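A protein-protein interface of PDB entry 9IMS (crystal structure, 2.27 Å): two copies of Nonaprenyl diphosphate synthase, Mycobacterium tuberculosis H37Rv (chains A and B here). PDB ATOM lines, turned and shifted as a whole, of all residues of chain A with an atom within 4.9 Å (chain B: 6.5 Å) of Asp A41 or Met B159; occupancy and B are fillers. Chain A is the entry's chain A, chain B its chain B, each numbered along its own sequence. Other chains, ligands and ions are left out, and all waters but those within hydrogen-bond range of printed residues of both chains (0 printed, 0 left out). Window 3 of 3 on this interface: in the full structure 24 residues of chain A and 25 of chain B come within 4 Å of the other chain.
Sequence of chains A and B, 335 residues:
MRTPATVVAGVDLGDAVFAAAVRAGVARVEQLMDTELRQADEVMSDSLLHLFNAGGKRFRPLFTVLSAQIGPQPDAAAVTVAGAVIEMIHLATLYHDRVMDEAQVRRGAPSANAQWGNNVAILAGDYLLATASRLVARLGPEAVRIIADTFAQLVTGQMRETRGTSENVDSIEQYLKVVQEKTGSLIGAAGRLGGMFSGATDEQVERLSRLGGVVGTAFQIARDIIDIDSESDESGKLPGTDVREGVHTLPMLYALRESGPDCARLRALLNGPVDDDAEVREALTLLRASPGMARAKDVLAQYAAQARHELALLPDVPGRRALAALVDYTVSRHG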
ATOM      1  N   GLN A  39       8.746  -9.786 -18.422  1.00  0.00           N
ATOM      2  CA  GLN A  39       9.533 -11.006 -18.564  1.00  0.00           C
ATOM      3  C   GLN A  39      10.567 -11.034 -17.438  1.00  0.00           C
ATOM      4  O   GLN A  39      10.463 -10.324 -16.426  1.00  0.00           O
ATOM      5  CB  GLN A  39      10.143 -11.093 -19.974  1.00  0.00           C
ATOM      6  CG  GLN A  39      11.343 -10.189 -20.282  1.00  0.00           C
ATOM      7  CD  GLN A  39      10.980  -8.834 -20.886  1.00  0.00           C
ATOM      8  OE1 GLN A  39      10.239  -8.754 -21.866  1.00  0.00           O
ATOM      9  NE2 GLN A  39      11.551  -7.763 -20.330  1.00  0.00           N
ATOM     10  N   ALA A  40      11.581 -11.878 -17.594  1.00  0.00           N
ATOM     11  CA  ALA A  40      12.692 -11.943 -16.646  1.00  0.00           C
ATOM     12  C   ALA A  40      13.887 -11.153 -17.182  1.00  0.00           C
ATOM     13  O   ALA A  40      14.952 -11.701 -17.496  1.00  0.00           O
ATOM     14  CB  ALA A  40      13.059 -13.396 -16.359  1.00  0.00           C
ATOM     15  N   ASP A  41      13.684  -9.838 -17.290  1.00  0.00           N
ATOM     16  CA  ASP A  41      14.682  -8.923 -17.857  1.00  0.00           C
ATOM     17  C   ASP A  41      14.616  -7.532 -17.230  1.00  0.00           C
ATOM     18  O   ASP A  41      14.185  -7.370 -16.093  1.00  0.00           O
ATOM     19  CB  ASP A  41      14.503  -8.796 -19.369  1.00  0.00           C
ATOM     20  CG  ASP A  41      14.856  -7.411 -19.879  1.00  0.00           C
ATOM     21  OD1 ASP A  41      16.058  -7.076 -19.889  1.00  0.00           O
ATOM     22  OD2 ASP A  41      13.936  -6.652 -20.262  1.00  0.00           O
ATOM     23  N   MET A  44      12.628  -1.840 -17.961  1.00  0.00           N
ATOM     24  CA  MET A  44      11.270  -2.388 -17.926  1.00  0.00           C
ATOM     25  C   MET A  44      10.201  -1.417 -17.416  1.00  0.00           C
ATOM     26  O   MET A  44       9.142  -1.823 -16.930  1.00  0.00           O
ATOM     27  CB  MET A  44      11.235  -3.669 -17.093  1.00  0.00           C
ATOM     28  CG  MET A  44      12.238  -4.703 -17.541  1.00  0.00           C
ATOM     29  SD  MET A  44      11.501  -6.323 -17.265  1.00  0.00           S
ATOM     30  CE  MET A  44       9.938  -6.128 -18.140  1.00  0.00           C
ATOM     31  N   LEU A 123      13.405  -1.129 -30.652  1.00  0.00           N
ATOM     32  CA  LEU A 123      13.235  -2.486 -30.138  1.00  0.00           C
ATOM     33  C   LEU A 123      12.001  -2.587 -29.250  1.00  0.00           C
ATOM     34  O   LEU A 123      11.214  -3.537 -29.366  1.00  0.00           O
ATOM     35  CB  LEU A 123      14.483  -2.918 -29.357  1.00  0.00           C
ATOM     36  CG  LEU A 123      15.783  -3.132 -30.142  1.00  0.00           C
ATOM     37  CD1 LEU A 123      16.902  -3.594 -29.221  1.00  0.00           C
ATOM     38  CD2 LEU A 123      15.583  -4.109 -31.319  1.00  0.00           C
ATOM     39  N   TYR A 127       8.910  -5.055 -29.756  1.00  0.00           N
ATOM     40  CA  TYR A 127       8.403  -6.009 -28.764  1.00  0.00           C
ATOM     41  C   TYR A 127       6.908  -5.814 -28.513  1.00  0.00           C
ATOM     42  O   TYR A 127       6.151  -6.787 -28.453  1.00  0.00           O
ATOM     43  CB  TYR A 127       9.181  -5.869 -27.459  1.00  0.00           C
ATOM     44  CG  TYR A 127       8.867  -6.947 -26.444  1.00  0.00           C
ATOM     45  CD1 TYR A 127       9.289  -8.260 -26.635  1.00  0.00           C
ATOM     46  CD2 TYR A 127       8.153  -6.649 -25.288  1.00  0.00           C
ATOM     47  CE1 TYR A 127       9.007  -9.247 -25.706  1.00  0.00           C
ATOM     48  CE2 TYR A 127       7.867  -7.628 -24.356  1.00  0.00           C
ATOM     49  CZ  TYR A 127       8.296  -8.921 -24.571  1.00  0.00           C
ATOM     50  OH  TYR A 127       8.005  -9.890 -23.649  1.00  0.00           O
ATOM     51  N   LEU B 154      13.213 -12.774 -30.529  1.00  0.00           N
ATOM     52  CA  LEU B 154      14.301 -12.168 -31.280  1.00  0.00           C
ATOM     53  C   LEU B 154      14.604 -10.767 -30.764  1.00  0.00           C
ATOM     54  O   LEU B 154      15.768 -10.350 -30.691  1.00  0.00           O
ATOM     55  CB  LEU B 154      13.888 -12.136 -32.747  1.00  0.00           C
ATOM     56  CG  LEU B 154      14.801 -12.348 -33.922  1.00  0.00           C
ATOM     57  CD1 LEU B 154      13.882 -12.521 -35.129  1.00  0.00           C
ATOM     58  CD2 LEU B 154      15.724 -11.151 -34.070  1.00  0.00           C
ATOM     59  N   VAL B 155      13.559 -10.036 -30.381  1.00  0.00           N
ATOM     60  CA  VAL B 155      13.723  -8.677 -29.873  1.00  0.00           C
ATOM     61  C   VAL B 155      14.321  -8.679 -28.467  1.00  0.00           C
ATOM     62  O   VAL B 155      15.224  -7.887 -28.172  1.00  0.00           O
ATOM     63  CB  VAL B 155      12.376  -7.937 -29.920  1.00  0.00           C
ATOM     64  CG1 VAL B 155      12.465  -6.625 -29.155  1.00  0.00           C
ATOM     65  CG2 VAL B 155      12.010  -7.669 -31.379  1.00  0.00           C
ATOM     66  N   THR B 156      13.805  -9.523 -27.562  1.00  0.00           N
ATOM     67  CA  THR B 156      14.382  -9.530 -26.215  1.00  0.00           C
ATOM     68  C   THR B 156      15.821 -10.009 -26.255  1.00  0.00           C
ATOM     69  O   THR B 156      16.654  -9.520 -25.485  1.00  0.00           O
ATOM     70  CB  THR B 156      13.566 -10.384 -25.226  1.00  0.00           C
ATOM     71  OG1 THR B 156      14.439 -11.118 -24.351  1.00  0.00           O
ATOM     72  CG2 THR B 156      12.721 -11.365 -25.905  1.00  0.00           C
ATOM     73  N   GLY B 157      16.142 -10.922 -27.178  1.00  0.00           N
ATOM     74  CA  GLY B 157      17.539 -11.241 -27.447  1.00  0.00           C
ATOM     75  C   GLY B 157      18.389 -10.012 -27.692  1.00  0.00           C
ATOM     76  O   GLY B 157      19.484  -9.886 -27.142  1.00  0.00           O
ATOM     77  N   GLN B 158      17.890  -9.073 -28.510  1.00  0.00           N
ATOM     78  CA  GLN B 158      18.656  -7.860 -28.792  1.00  0.00           C
ATOM     79  C   GLN B 158      18.635  -6.892 -27.612  1.00  0.00           C
ATOM     80  O   GLN B 158      19.621  -6.184 -27.370  1.00  0.00           O
ATOM     81  CB  GLN B 158      18.132  -7.177 -30.057  1.00  0.00           C
ATOM     82  CG  GLN B 158      18.202  -8.026 -31.328  1.00  0.00           C
ATOM     83  CD  GLN B 158      18.246  -7.169 -32.600  1.00  0.00           C
ATOM     84  OE1 GLN B 158      17.925  -5.979 -32.570  1.00  0.00           O
ATOM     85  NE2 GLN B 158      18.641  -7.777 -33.722  1.00  0.00           N
ATOM     86  N   MET B 159      17.515  -6.809 -26.890  1.00  0.00           N
ATOM     87  CA  MET B 159      17.521  -6.096 -25.616  1.00  0.00           C
ATOM     88  C   MET B 159      18.539  -6.714 -24.662  1.00  0.00           C
ATOM     89  O   MET B 159      19.403  -6.014 -24.115  1.00  0.00           O
ATOM     90  CB  MET B 159      16.116  -6.085 -24.976  1.00  0.00           C
ATOM     91  CG  MET B 159      15.078  -5.069 -25.563  1.00  0.00           C
ATOM     92  SD  MET B 159      13.278  -5.428 -25.407  1.00  0.00           S
ATOM     93  CE  MET B 159      13.170  -6.311 -23.851  1.00  0.00           C
ATOM     94  N   ARG B 160      18.458  -8.036 -24.457  1.00  0.00           N
ATOM     95  CA  ARG B 160      19.341  -8.687 -23.493  1.00  0.00           C
ATOM     96  C   ARG B 160      20.803  -8.494 -23.856  1.00  0.00           C
ATOM     97  O   ARG B 160      21.648  -8.331 -22.969  1.00  0.00           O
ATOM     98  CB  ARG B 160      19.029 -10.180 -23.394  1.00  0.00           C
ATOM     99  CG  ARG B 160      19.555 -10.824 -22.123  1.00  0.00           C
ATOM    100  CD  ARG B 160      19.427 -12.337 -22.192  1.00  0.00           C
ATOM    101  NE  ARG B 160      18.038 -12.773 -22.259  1.00  0.00           N
ATOM    102  CZ  ARG B 160      17.247 -12.917 -21.204  1.00  0.00           C
ATOM    103  NH1 ARG B 160      17.664 -12.620 -19.987  1.00  0.00           N
ATOM    104  NH2 ARG B 160      16.015 -13.383 -21.377  1.00  0.00           N
ATOM    105  N   GLU B 161      21.125  -8.507 -25.157  1.00  0.00           N
ATOM    106  CA  GLU B 161      22.503  -8.276 -25.582  1.00  0.00           C
ATOM    107  C   GLU B 161      22.998  -6.906 -25.143  1.00  0.00           C
ATOM    108  O   GLU B 161      24.204  -6.711 -24.956  1.00  0.00           O
ATOM    109  CB  GLU B 161      22.626  -8.416 -27.101  1.00  0.00           C
ATOM    110  CG  GLU B 161      24.066  -8.309 -27.623  1.00  0.00           C
ATOM    111  CD  GLU B 161      24.167  -8.532 -29.124  1.00  0.00           C
ATOM    112  OE1 GLU B 161      24.072  -7.545 -29.894  1.00  0.00           O
ATOM    113  OE2 GLU B 161      24.339  -9.694 -29.537  1.00  0.00           O
ATOM    114  N   THR B 162      22.093  -5.953 -24.966  1.00  0.00           N
ATOM    115  CA  THR B 162      22.493  -4.610 -24.568  1.00  0.00           C
ATOM    116  C   THR B 162      22.478  -4.448 -23.049  1.00  0.00           C
ATOM    117  O   THR B 162      23.300  -5.039 -22.340  1.00  0.00           O
ATOM    118  CB  THR B 162      21.582  -3.552 -25.211  1.00  0.00           C
ATOM    119  OG1 THR B 162      22.024  -3.302 -26.554  1.00  0.00           O
ATOM    120  CG2 THR B 162      21.608  -2.258 -24.402  1.00  0.00           C
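The side-chain carboxylate of Asp A41 lies within hydrogen-bond range of the side-chain amide nitrogen of Gln A39, 2.6 Å away.
The side-chain hydroxyl of Tyr A127 is in hydrogen-bond range of the side-chain amide oxygen of Gln A39 (3.1 Å).
Arg B160 touches Ala A40 (NH1 to O, 3.8 Å).
Met B159 touches Asp A41.
Val B155 touches Leu A123.
CD2 of Leu A123 touches OE1 of Gln B158 (3.2 Å).
Tyr A127 touches Val B155.
Of chain B, only Met B159 comes within 4 Å of Asp A41.
Of the printed residues of chain B, Leu A123 touches Val B155 (3.3 Å) and Gln B158 (3.2 Å).
Of the printed residues of chain B, Tyr A127 touches Val B155.
Leu B154 touches none of the printed residues of chain A.
Of the printed residues of chain A, Gln B158 touches Leu A123 (3.2 Å).
Printed residues of chain A within 4 Å of Met B159: Asp A41.
Of the printed residues of chain A, Arg B160 touches Ala A40.
The nearest residue of chain B that does not touch Asp A41 is Arg B160 (5.0 Å).
The nearest printed residue of chain A that does not touch Met B159 is Leu A123 (4.02 Å).
The nearest printed residue of chain A that does not touch Val B155 is Gln A39 (7.8 Å).
Printed residues of chain B that touch a printed residue of chain A: Val B155, Gln B158, Met B159 and Arg B160.
Hydrophobic or aromatic side chains of chain B within 4 Å of the printed part of chain A: Val B155 and Met B159.
Along chain A the printed residues that touch a printed residue of chain B span positions 40 to 127.
No position is printed for both chains.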
